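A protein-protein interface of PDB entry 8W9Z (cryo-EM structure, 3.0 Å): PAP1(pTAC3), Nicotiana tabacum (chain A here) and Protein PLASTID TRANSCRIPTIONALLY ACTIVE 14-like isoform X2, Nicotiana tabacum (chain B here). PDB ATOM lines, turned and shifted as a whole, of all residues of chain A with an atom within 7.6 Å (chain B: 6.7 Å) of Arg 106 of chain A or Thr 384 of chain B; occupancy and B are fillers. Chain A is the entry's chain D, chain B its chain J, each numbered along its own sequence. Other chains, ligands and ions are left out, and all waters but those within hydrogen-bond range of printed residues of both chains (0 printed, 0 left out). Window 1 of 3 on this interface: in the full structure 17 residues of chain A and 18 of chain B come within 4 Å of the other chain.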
ATOM      1  N   MET A  74     -24.157  18.109 -31.671  1.00  0.00           N
ATOM      2  CA  MET A  74     -25.229  17.923 -30.701  1.00  0.00           C
ATOM      3  C   MET A  74     -25.727  19.227 -30.088  1.00  0.00           C
ATOM      4  O   MET A  74     -26.898  19.298 -29.693  1.00  0.00           O
ATOM      5  CB  MET A  74     -24.772  16.976 -29.586  1.00  0.00           C
ATOM      6  CG  MET A  74     -25.896  16.489 -28.683  1.00  0.00           C
ATOM      7  SD  MET A  74     -25.391  15.165 -27.568  1.00  0.00           S
ATOM      8  CE  MET A  74     -24.894  13.905 -28.740  1.00  0.00           C
ATOM      9  N   LEU A  77     -28.328  20.779 -32.320  1.00  0.00           N
ATOM     10  CA  LEU A  77     -29.451  19.847 -32.329  1.00  0.00           C
ATOM     11  C   LEU A  77     -30.324  20.038 -31.095  1.00  0.00           C
ATOM     12  O   LEU A  77     -31.550  20.166 -31.197  1.00  0.00           O
ATOM     13  CB  LEU A  77     -28.936  18.408 -32.419  1.00  0.00           C
ATOM     14  CG  LEU A  77     -29.947  17.265 -32.546  1.00  0.00           C
ATOM     15  CD1 LEU A  77     -29.372  16.150 -33.402  1.00  0.00           C
ATOM     16  CD2 LEU A  77     -30.344  16.719 -31.182  1.00  0.00           C
ATOM     17  N   MET A  78     -29.703  20.065 -29.913  1.00  0.00           N
ATOM     18  CA  MET A  78     -30.462  20.291 -28.687  1.00  0.00           C
ATOM     19  C   MET A  78     -31.074  21.685 -28.652  1.00  0.00           C
ATOM     20  O   MET A  78     -32.186  21.859 -28.139  1.00  0.00           O
ATOM     21  CB  MET A  78     -29.568  20.074 -27.466  1.00  0.00           C
ATOM     22  CG  MET A  78     -29.044  18.655 -27.325  1.00  0.00           C
ATOM     23  SD  MET A  78     -30.367  17.436 -27.214  1.00  0.00           S
ATOM     24  CE  MET A  78     -29.419  15.932 -27.005  1.00  0.00           C
ATOM     25  N   MET A  96     -25.675  14.881 -40.036  1.00  0.00           N
ATOM     26  CA  MET A  96     -24.671  14.173 -39.251  1.00  0.00           C
ATOM     27  C   MET A  96     -24.509  12.725 -39.696  1.00  0.00           C
ATOM     28  O   MET A  96     -23.415  12.166 -39.563  1.00  0.00           O
ATOM     29  CB  MET A  96     -25.012  14.237 -37.760  1.00  0.00           C
ATOM     30  CG  MET A  96     -26.193  13.385 -37.343  1.00  0.00           C
ATOM     31  SD  MET A  96     -26.481  13.402 -35.566  1.00  0.00           S
ATOM     32  CE  MET A  96     -27.853  12.259 -35.451  1.00  0.00           C
ATOM     33  N   PRO A 103     -25.659   7.767 -35.911  1.00  0.00           N
ATOM     34  CA  PRO A 103     -26.402   8.460 -34.855  1.00  0.00           C
ATOM     35  C   PRO A 103     -26.428   7.650 -33.569  1.00  0.00           C
ATOM     36  O   PRO A 103     -26.433   6.417 -33.580  1.00  0.00           O
ATOM     37  CB  PRO A 103     -27.808   8.606 -35.448  1.00  0.00           C
ATOM     38  CG  PRO A 103     -27.917   7.477 -36.417  1.00  0.00           C
ATOM     39  CD  PRO A 103     -26.541   7.300 -36.994  1.00  0.00           C
ATOM     40  N   GLY A 104     -26.445   8.366 -32.449  1.00  0.00           N
ATOM     41  CA  GLY A 104     -26.470   7.743 -31.149  1.00  0.00           C
ATOM     42  C   GLY A 104     -27.795   7.945 -30.442  1.00  0.00           C
ATOM     43  O   GLY A 104     -28.705   8.603 -30.955  1.00  0.00           O
ATOM     44  N   PRO A 105     -27.926   7.378 -29.240  1.00  0.00           N
ATOM     45  CA  PRO A 105     -29.192   7.542 -28.507  1.00  0.00           C
ATOM     46  C   PRO A 105     -29.404   8.957 -28.004  1.00  0.00           C
ATOM     47  O   PRO A 105     -30.547   9.430 -27.964  1.00  0.00           O
ATOM     48  CB  PRO A 105     -29.058   6.535 -27.357  1.00  0.00           C
ATOM     49  CG  PRO A 105     -27.587   6.405 -27.149  1.00  0.00           C
ATOM     50  CD  PRO A 105     -26.964   6.535 -28.511  1.00  0.00           C
ATOM     51  N   ARG A 106     -28.330   9.651 -27.616  1.00  0.00           N
ATOM     52  CA  ARG A 106     -28.465  11.032 -27.172  1.00  0.00           C
ATOM     53  C   ARG A 106     -28.992  11.927 -28.284  1.00  0.00           C
ATOM     54  O   ARG A 106     -29.760  12.859 -28.019  1.00  0.00           O
ATOM     55  CB  ARG A 106     -27.121  11.555 -26.664  1.00  0.00           C
ATOM     56  CG  ARG A 106     -26.553  10.773 -25.493  1.00  0.00           C
ATOM     57  CD  ARG A 106     -27.439  10.899 -24.267  1.00  0.00           C
ATOM     58  NE  ARG A 106     -27.010  10.016 -23.188  1.00  0.00           N
ATOM     59  CZ  ARG A 106     -26.160  10.366 -22.229  1.00  0.00           C
ATOM     60  NH1 ARG A 106     -25.644  11.587 -22.212  1.00  0.00           N
ATOM     61  NH2 ARG A 106     -25.826   9.496 -21.286  1.00  0.00           N
ATOM     62  N   SER A 107     -28.599  11.658 -29.530  1.00  0.00           N
ATOM     63  CA  SER A 107     -29.076  12.465 -30.648  1.00  0.00           C
ATOM     64  C   SER A 107     -30.546  12.190 -30.934  1.00  0.00           C
ATOM     65  O   SER A 107     -31.329  13.120 -31.163  1.00  0.00           O
ATOM     66  CB  SER A 107     -28.223  12.195 -31.887  1.00  0.00           C
ATOM     67  OG  SER A 107     -28.283  10.830 -32.259  1.00  0.00           O
ATOM     68  N   PHE A 108     -30.941  10.915 -30.932  1.00  0.00           N
ATOM     69  CA  PHE A 108     -32.338  10.568 -31.160  1.00  0.00           C
ATOM     70  C   PHE A 108     -33.239  11.010 -30.016  1.00  0.00           C
ATOM     71  O   PHE A 108     -34.450  11.157 -30.219  1.00  0.00           O
ATOM     72  CB  PHE A 108     -32.477   9.062 -31.385  1.00  0.00           C
ATOM     73  CG  PHE A 108     -32.065   8.615 -32.756  1.00  0.00           C
ATOM     74  CD1 PHE A 108     -32.168   9.473 -33.838  1.00  0.00           C
ATOM     75  CD2 PHE A 108     -31.575   7.338 -32.965  1.00  0.00           C
ATOM     76  CE1 PHE A 108     -31.790   9.065 -35.103  1.00  0.00           C
ATOM     77  CE2 PHE A 108     -31.195   6.924 -34.227  1.00  0.00           C
ATOM     78  CZ  PHE A 108     -31.304   7.789 -35.298  1.00  0.00           C
ATOM     79  N   HIS A 109     -32.680  11.220 -28.822  1.00  0.00           N
ATOM     80  CA  HIS A 109     -33.477  11.748 -27.721  1.00  0.00           C
ATOM     81  C   HIS A 109     -34.066  13.109 -28.071  1.00  0.00           C
ATOM     82  O   HIS A 109     -35.230  13.389 -27.765  1.00  0.00           O
ATOM     83  CB  HIS A 109     -32.628  11.841 -26.454  1.00  0.00           C
ATOM     84  CG  HIS A 109     -33.276  12.617 -25.350  1.00  0.00           C
ATOM     85  ND1 HIS A 109     -34.545  12.338 -24.891  1.00  0.00           N
ATOM     86  CD2 HIS A 109     -32.833  13.666 -24.618  1.00  0.00           C
ATOM     87  CE1 HIS A 109     -34.856  13.182 -23.924  1.00  0.00           C
ATOM     88  NE2 HIS A 109     -33.833  13.997 -23.737  1.00  0.00           N
ATOM     89  N   GLY A 110     -33.277  13.967 -28.721  1.00  0.00           N
ATOM     90  CA  GLY A 110     -33.791  15.262 -29.130  1.00  0.00           C
ATOM     91  C   GLY A 110     -34.867  15.149 -30.191  1.00  0.00           C
ATOM     92  O   GLY A 110     -35.866  15.874 -30.157  1.00  0.00           O
ATOM     93  N   PHE A 111     -34.687  14.232 -31.145  1.00  0.00           N
ATOM     94  CA  PHE A 111     -35.697  14.036 -32.179  1.00  0.00           C
ATOM     95  C   PHE A 111     -36.995  13.495 -31.597  1.00  0.00           C
ATOM     96  O   PHE A 111     -38.077  13.796 -32.113  1.00  0.00           O
ATOM     97  CB  PHE A 111     -35.160  13.099 -33.261  1.00  0.00           C
ATOM     98  CG  PHE A 111     -36.019  13.036 -34.490  1.00  0.00           C
ATOM     99  CD1 PHE A 111     -36.093  14.115 -35.355  1.00  0.00           C
ATOM    100  CD2 PHE A 111     -36.740  11.894 -34.790  1.00  0.00           C
ATOM    101  CE1 PHE A 111     -36.880  14.058 -36.490  1.00  0.00           C
ATOM    102  CE2 PHE A 111     -37.529  11.831 -35.922  1.00  0.00           C
ATOM    103  CZ  PHE A 111     -37.599  12.914 -36.774  1.00  0.00           C
ATOM    104  N   VAL A 112     -36.910  12.703 -30.528  1.00  0.00           N
ATOM    105  CA  VAL A 112     -38.121  12.206 -29.880  1.00  0.00           C
ATOM    106  C   VAL A 112     -38.789  13.318 -29.078  1.00  0.00           C
ATOM    107  O   VAL A 112     -40.010  13.506 -29.142  1.00  0.00           O
ATOM    108  CB  VAL A 112     -37.800  10.986 -28.999  1.00  0.00           C
ATOM    109  CG1 VAL A 112     -39.015  10.588 -28.181  1.00  0.00           C
ATOM    110  CG2 VAL A 112     -37.339   9.823 -29.860  1.00  0.00           C
ATOM    111  N   GLU A 131     -35.113   4.694 -34.226  1.00  0.00           N
ATOM    112  CA  GLU A 131     -34.005   4.419 -33.318  1.00  0.00           C
ATOM    113  C   GLU A 131     -33.828   2.921 -33.095  1.00  0.00           C
ATOM    114  O   GLU A 131     -32.698   2.431 -32.983  1.00  0.00           O
ATOM    115  CB  GLU A 131     -34.228   5.140 -31.988  1.00  0.00           C
ATOM    116  CG  GLU A 131     -33.120   4.927 -30.968  1.00  0.00           C
ATOM    117  CD  GLU A 131     -33.309   5.768 -29.721  1.00  0.00           C
ATOM    118  OE1 GLU A 131     -34.374   6.406 -29.587  1.00  0.00           O
ATOM    119  OE2 GLU A 131     -32.389   5.794 -28.877  1.00  0.00           O
ATOM    120  N   LEU A 136     -30.153  -0.292 -31.808  1.00  0.00           N
ATOM    121  CA  LEU A 136     -29.691   0.494 -30.673  1.00  0.00           C
ATOM    122  C   LEU A 136     -30.842   0.648 -29.691  1.00  0.00           C
ATOM    123  O   LEU A 136     -31.921   1.120 -30.062  1.00  0.00           O
ATOM    124  CB  LEU A 136     -29.179   1.868 -31.122  1.00  0.00           C
ATOM    125  CG  LEU A 136     -27.999   2.488 -30.366  1.00  0.00           C
ATOM    126  CD1 LEU A 136     -27.545   3.767 -31.053  1.00  0.00           C
ATOM    127  CD2 LEU A 136     -28.339   2.760 -28.907  1.00  0.00           C
ATOM    128  N   LEU A 139     -32.805   5.127 -24.634  1.00  0.00           N
ATOM    129  CA  LEU A 139     -32.493   5.479 -23.260  1.00  0.00           C
ATOM    130  C   LEU A 139     -33.753   5.441 -22.397  1.00  0.00           C
ATOM    131  O   LEU A 139     -34.868   5.223 -22.876  1.00  0.00           O
ATOM    132  CB  LEU A 139     -31.845   6.859 -23.198  1.00  0.00           C
ATOM    133  CG  LEU A 139     -30.552   7.016 -23.996  1.00  0.00           C
ATOM    134  CD1 LEU A 139     -30.042   8.443 -23.900  1.00  0.00           C
ATOM    135  CD2 LEU A 139     -29.500   6.034 -23.509  1.00  0.00           C
ATOM    136  N   GLU A 141     -34.886   8.052 -20.522  1.00  0.00           N
ATOM    137  CA  GLU A 141     -35.626   9.309 -20.585  1.00  0.00           C
ATOM    138  C   GLU A 141     -36.568   9.341 -21.782  1.00  0.00           C
ATOM    139  O   GLU A 141     -37.678   9.878 -21.691  1.00  0.00           O
ATOM    140  CB  GLU A 141     -34.652  10.487 -20.625  1.00  0.00           C
ATOM    141  CG  GLU A 141     -35.308  11.843 -20.846  1.00  0.00           C
ATOM    142  CD  GLU A 141     -36.261  12.234 -19.733  1.00  0.00           C
ATOM    143  OE1 GLU A 141     -36.098  11.737 -18.599  1.00  0.00           O
ATOM    144  OE2 GLU A 141     -37.177  13.044 -19.992  1.00  0.00           O
ATOM    145  N   THR A 142     -36.149   8.764 -22.909  1.00  0.00           N
ATOM    146  CA  THR A 142     -37.018   8.717 -24.081  1.00  0.00           C
ATOM    147  C   THR A 142     -38.268   7.891 -23.801  1.00  0.00           C
ATOM    148  O   THR A 142     -39.389   8.313 -24.110  1.00  0.00           O
ATOM    149  CB  THR A 142     -36.256   8.147 -25.279  1.00  0.00           C
ATOM    150  OG1 THR A 142     -35.848   6.804 -24.992  1.00  0.00           O
ATOM    151  CG2 THR A 142     -35.025   8.991 -25.575  1.00  0.00           C
ATOM    152  N   HIS B 381     -27.568  18.409 -14.777  1.00  0.00           N
ATOM    153  CA  HIS B 381     -28.805  17.705 -15.080  1.00  0.00           C
ATOM    154  C   HIS B 381     -28.829  16.360 -14.364  1.00  0.00           C
ATOM    155  O   HIS B 381     -27.825  15.644 -14.323  1.00  0.00           O
ATOM    156  CB  HIS B 381     -28.956  17.503 -16.587  1.00  0.00           C
ATOM    157  CG  HIS B 381     -30.349  17.156 -17.012  1.00  0.00           C
ATOM    158  ND1 HIS B 381     -31.363  18.087 -17.065  1.00  0.00           N
ATOM    159  CD2 HIS B 381     -30.897  15.981 -17.399  1.00  0.00           C
ATOM    160  CE1 HIS B 381     -32.476  17.502 -17.468  1.00  0.00           C
ATOM    161  NE2 HIS B 381     -32.220  16.224 -17.679  1.00  0.00           N
ATOM    162  N   LEU B 382     -29.988  16.019 -13.801  1.00  0.00           N
ATOM    163  CA  LEU B 382     -30.109  14.837 -12.955  1.00  0.00           C
ATOM    164  C   LEU B 382     -30.419  13.573 -13.750  1.00  0.00           C
ATOM    165  O   LEU B 382     -29.783  12.534 -13.538  1.00  0.00           O
ATOM    166  CB  LEU B 382     -31.190  15.062 -11.894  1.00  0.00           C
ATOM    167  CG  LEU B 382     -31.451  13.892 -10.944  1.00  0.00           C
ATOM    168  CD1 LEU B 382     -30.185  13.518 -10.190  1.00  0.00           C
ATOM    169  CD2 LEU B 382     -32.576  14.227  -9.977  1.00  0.00           C
ATOM    170  N   ASP B 383     -31.394  13.638 -14.658  1.00  0.00           N
ATOM    171  CA  ASP B 383     -31.826  12.432 -15.355  1.00  0.00           C
ATOM    172  C   ASP B 383     -30.746  11.919 -16.298  1.00  0.00           C
ATOM    173  O   ASP B 383     -30.509  10.708 -16.379  1.00  0.00           O
ATOM    174  CB  ASP B 383     -33.127  12.699 -16.111  1.00  0.00           C
ATOM    175  CG  ASP B 383     -33.921  11.433 -16.369  1.00  0.00           C
ATOM    176  OD1 ASP B 383     -33.346  10.463 -16.904  1.00  0.00           O
ATOM    177  OD2 ASP B 383     -35.120  11.404 -16.020  1.00  0.00           O
ATOM    178  N   THR B 384     -30.071  12.823 -17.011  1.00  0.00           N
ATOM    179  CA  THR B 384     -28.961  12.404 -17.861  1.00  0.00           C
ATOM    180  C   THR B 384     -27.819  11.836 -17.026  1.00  0.00           C
ATOM    181  O   THR B 384     -27.171  10.859 -17.424  1.00  0.00           O
ATOM    182  CB  THR B 384     -28.476  13.579 -18.709  1.00  0.00           C
ATOM    183  OG1 THR B 384     -29.570  14.100 -19.475  1.00  0.00           O
ATOM    184  CG2 THR B 384     -27.372  13.136 -19.659  1.00  0.00           C
ATOM    185  N   PHE B 385     -27.572  12.426 -15.853  1.00  0.00           N
ATOM    186  CA  PHE B 385     -26.510  11.937 -14.979  1.00  0.00           C
ATOM    187  C   PHE B 385     -26.824  10.548 -14.440  1.00  0.00           C
ATOM    188  O   PHE B 385     -25.910   9.740 -14.243  1.00  0.00           O
ATOM    189  CB  PHE B 385     -26.290  12.915 -13.827  1.00  0.00           C
ATOM    190  CG  PHE B 385     -25.000  12.707 -13.090  1.00  0.00           C
ATOM    191  CD1 PHE B 385     -24.927  11.831 -12.024  1.00  0.00           C
ATOM    192  CD2 PHE B 385     -23.859  13.397 -13.463  1.00  0.00           C
ATOM    193  CE1 PHE B 385     -23.743  11.642 -11.346  1.00  0.00           C
ATOM    194  CE2 PHE B 385     -22.670  13.212 -12.787  1.00  0.00           C
ATOM    195  CZ  PHE B 385     -22.612  12.333 -11.727  1.00  0.00           C
ATOM    196  N   LEU B 386     -28.099  10.255 -14.186  1.00  0.00           N
ATOM    197  CA  LEU B 386     -28.472   8.916 -13.750  1.00  0.00           C
ATOM    198  C   LEU B 386     -28.487   7.925 -14.905  1.00  0.00           C
ATOM    199  O   LEU B 386     -28.216   6.737 -14.701  1.00  0.00           O
ATOM    200  CB  LEU B 386     -29.841   8.943 -13.067  1.00  0.00           C
ATOM    201  CG  LEU B 386     -29.952   9.756 -11.777  1.00  0.00           C
ATOM    202  CD1 LEU B 386     -31.366   9.694 -11.226  1.00  0.00           C
ATOM    203  CD2 LEU B 386     -28.950   9.264 -10.746  1.00  0.00           C
ATOM    204  N   SER B 387     -28.793   8.392 -16.118  1.00  0.00           N
ATOM    205  CA  SER B 387     -28.837   7.491 -17.264  1.00  0.00           C
ATOM    206  C   SER B 387     -27.437   7.108 -17.726  1.00  0.00           C
ATOM    207  O   SER B 387     -27.214   5.979 -18.178  1.00  0.00           O
ATOM    208  CB  SER B 387     -29.620   8.135 -18.407  1.00  0.00           C
ATOM    209  OG  SER B 387     -29.679   7.276 -19.532  1.00  0.00           O
ATOM    210  N   VAL B 388     -26.479   8.033 -17.623  1.00  0.00           N
ATOM    211  CA  VAL B 388     -25.128   7.737 -18.089  1.00  0.00           C
ATOM    212  C   VAL B 388     -24.429   6.758 -17.152  1.00  0.00           C
ATOM    213  O   VAL B 388     -23.590   5.962 -17.591  1.00  0.00           O
ATOM    214  CB  VAL B 388     -24.323   9.040 -18.262  1.00  0.00           C
ATOM    215  CG1 VAL B 388     -24.147   9.749 -16.932  1.00  0.00           C
ATOM    216  CG2 VAL B 388     -22.974   8.758 -18.908  1.00  0.00           C
ATOM    217  N   PHE B 389     -24.764   6.782 -15.863  1.00  0.00           N
ATOM    218  CA  PHE B 389     -24.148   5.898 -14.882  1.00  0.00           C
ATOM    219  C   PHE B 389     -25.011   4.688 -14.551  1.00  0.00           C
ATOM    220  O   PHE B 389     -24.679   3.941 -13.625  1.00  0.00           O
ATOM    221  CB  PHE B 389     -23.822   6.669 -13.603  1.00  0.00           C
ATOM    222  CG  PHE B 389     -22.624   7.565 -13.724  1.00  0.00           C
ATOM    223  CD1 PHE B 389     -21.351   7.029 -13.793  1.00  0.00           C
ATOM    224  CD2 PHE B 389     -22.770   8.939 -13.761  1.00  0.00           C
ATOM    225  CE1 PHE B 389     -20.245   7.849 -13.903  1.00  0.00           C
ATOM    226  CE2 PHE B 389     -21.670   9.763 -13.869  1.00  0.00           C
ATOM    227  CZ  PHE B 389     -20.407   9.218 -13.940  1.00  0.00           C
ATOM    228  N   PRO B 432     -34.797  18.792 -22.999  1.00  0.00           N
ATOM    229  CA  PRO B 432     -33.491  18.167 -23.176  1.00  0.00           C
ATOM    230  C   PRO B 432     -32.380  19.114 -22.767  1.00  0.00           C
ATOM    231  O   PRO B 432     -32.485  20.338 -22.957  1.00  0.00           O
ATOM    232  CB  PRO B 432     -33.447  17.866 -24.684  1.00  0.00           C
ATOM    233  CG  PRO B 432     -34.322  18.909 -25.284  1.00  0.00           C
ATOM    234  CD  PRO B 432     -35.423  19.153 -24.284  1.00  0.00           C
ATOM    235  N   PRO B 433     -31.292  18.597 -22.205  1.00  0.00           N
ATOM    236  CA  PRO B 433     -30.204  19.470 -21.760  1.00  0.00           C
ATOM    237  C   PRO B 433     -29.369  19.979 -22.924  1.00  0.00           C
ATOM    238  O   PRO B 433     -29.263  19.345 -23.977  1.00  0.00           O
ATOM    239  CB  PRO B 433     -29.375  18.555 -20.851  1.00  0.00           C
ATOM    240  CG  PRO B 433     -29.594  17.194 -21.418  1.00  0.00           C
ATOM    241  CD  PRO B 433     -31.016  17.177 -21.924  1.00  0.00           C
ATOM    242  N   TYR B 501     -18.859  12.091 -16.952  1.00  0.00           N
ATOM    243  CA  TYR B 501     -20.124  12.628 -17.439  1.00  0.00           C
ATOM    244  C   TYR B 501     -19.905  13.668 -18.529  1.00  0.00           C
ATOM    245  O   TYR B 501     -20.638  13.694 -19.525  1.00  0.00           O
ATOM    246  CB  TYR B 501     -20.925  13.228 -16.285  1.00  0.00           C
ATOM    247  CG  TYR B 501     -22.191  13.930 -16.727  1.00  0.00           C
ATOM    248  CD1 TYR B 501     -23.329  13.207 -17.050  1.00  0.00           C
ATOM    249  CD2 TYR B 501     -22.244  15.314 -16.821  1.00  0.00           C
ATOM    250  CE1 TYR B 501     -24.486  13.841 -17.456  1.00  0.00           C
ATOM    251  CE2 TYR B 501     -23.397  15.957 -17.227  1.00  0.00           C
ATOM    252  CZ  TYR B 501     -24.515  15.217 -17.542  1.00  0.00           C
ATOM    253  OH  TYR B 501     -25.665  15.853 -17.946  1.00  0.00           O
ATOM    254  N   ARG B 504     -18.696  11.749 -21.733  1.00  0.00           N
ATOM    255  CA  ARG B 504     -19.548  10.699 -22.273  1.00  0.00           C
ATOM    256  C   ARG B 504     -20.957  11.180 -22.596  1.00  0.00           C
ATOM    257  O   ARG B 504     -21.762  10.398 -23.110  1.00  0.00           O
ATOM    258  CB  ARG B 504     -19.610   9.517 -21.297  1.00  0.00           C
ATOM    259  CG  ARG B 504     -19.965   8.185 -21.946  1.00  0.00           C
ATOM    260  CD  ARG B 504     -19.911   7.046 -20.944  1.00  0.00           C
ATOM    261  NE  ARG B 504     -18.564   6.842 -20.421  1.00  0.00           N
ATOM    262  CZ  ARG B 504     -18.239   5.897 -19.545  1.00  0.00           C
ATOM    263  NH1 ARG B 504     -19.166   5.065 -19.090  1.00  0.00           N
ATOM    264  NH2 ARG B 504     -16.987   5.784 -19.123  1.00  0.00           N
ATOM    265  N   ILE B 505     -21.277  12.446 -22.318  1.00  0.00           N
ATOM    266  CA  ILE B 505     -22.592  12.966 -22.669  1.00  0.00           C
ATOM    267  C   ILE B 505     -22.741  13.125 -24.177  1.00  0.00           C
ATOM    268  O   ILE B 505     -23.865  13.121 -24.692  1.00  0.00           O
ATOM    269  CB  ILE B 505     -22.848  14.301 -21.940  1.00  0.00           C
ATOM    270  CG1 ILE B 505     -24.300  14.751 -22.116  1.00  0.00           C
ATOM    271  CG2 ILE B 505     -21.890  15.376 -22.429  1.00  0.00           C
ATOM    272  CD1 ILE B 505     -24.614  16.067 -21.444  1.00  0.00           C
ATOM    273  N   LEU B 506     -21.633  13.240 -24.904  1.00  0.00           N
ATOM    274  CA  LEU B 506     -21.636  13.396 -26.356  1.00  0.00           C
ATOM    275  C   LEU B 506     -21.146  12.083 -26.961  1.00  0.00           C
ATOM    276  O   LEU B 506     -19.953  11.901 -27.207  1.00  0.00           O
ATOM    277  CB  LEU B 506     -20.757  14.569 -26.782  1.00  0.00           C
ATOM    278  CG  LEU B 506     -20.927  15.871 -25.999  1.00  0.00           C
ATOM    279  CD1 LEU B 506     -19.928  16.913 -26.472  1.00  0.00           C
ATOM    280  CD2 LEU B 506     -22.348  16.395 -26.118  1.00  0.00           C
ATOM    281  N   PHE B 507     -22.078  11.165 -27.197  1.00  0.00           N
ATOM    282  CA  PHE B 507     -21.741   9.861 -27.756  1.00  0.00           C
ATOM    283  C   PHE B 507     -21.320   9.984 -29.217  1.00  0.00           C
ATOM    284  O   PHE B 507     -20.418   9.281 -29.673  1.00  0.00           O
ATOM    285  CB  PHE B 507     -22.924   8.900 -27.627  1.00  0.00           C
ATOM    286  CG  PHE B 507     -22.660   7.533 -28.193  1.00  0.00           C
ATOM    287  CD1 PHE B 507     -21.938   6.598 -27.469  1.00  0.00           C
ATOM    288  CD2 PHE B 507     -23.139   7.181 -29.443  1.00  0.00           C
ATOM    289  CE1 PHE B 507     -21.695   5.339 -27.986  1.00  0.00           C
ATOM    290  CE2 PHE B 507     -22.899   5.924 -29.965  1.00  0.00           C
ATOM    291  CZ  PHE B 507     -22.176   5.002 -29.235  1.00  0.00           C
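OE1 of Glu 141 of chain A lies close to OD2 of Asp 383 of chain B. The backbone carbonyl oxygen (O) of Ile 505 of chain B sits close to the guanidinium group (NH1) of Arg 106 of chain A (3.4 Å).
The backbone carbonyl oxygen (O) of Gly 104 of chain A is in hydrogen-bond range of the side-chain hydroxyl (OG) of Ser 107 of chain A.
Among the printed residues, merely in contact across the chains: Arg 106 of chain A with Val 388 of chain B (3.4 Å), Met 78 of chain A with Pro 433 of chain B (3.4 Å), Arg 106 of chain A with Thr 384 of chain B (3.5 Å), Met 74 of chain A with Leu 506 of chain B (3.6 Å), Gly 104 of chain A with Phe 507 of chain B (3.8 Å), Met 74 of chain A with Ile 505 of chain B (3.8 Å) and Pro 105 of chain A with Phe 507 of chain B (3.99 Å).
Arg 106 of chain A touches just these residues of chain B: Thr 384, Val 388 and Ile 505. Printed residues of chain A within 4 Å of Thr 384 of chain B: Arg 106. Of the printed residues of chain A, Ile 505 of chain B touches Met 74 and Arg 106. Printed residues of chain A within 4 Å of Phe 507 of chain B: Gly 104 and Pro 105. The nearest residue of chain B that does not touch Arg 106 of chain A is Arg 504 of chain B (4.2 Å). The nearest residue of chain A that does not touch Thr 384 of chain B is His 109 of chain A (6.0 Å). The nearest printed residue of chain B that does not touch Glu 141 of chain A is Ser 387 of chain B (5.4 Å).
Hydrophobic or aromatic side chains of chain B that line the printed part of chain A: Val 388, Ile 505, Leu 506 and Phe 507. Hydrophobic or aromatic side chains of chain A within 4 Å of the printed part of chain B: Met 74, Met 78 and Pro 105. Among the printed residues, no Asp or Glu carboxylate lies within 4 Å of a Lys or Arg side-chain nitrogen of the other chain.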
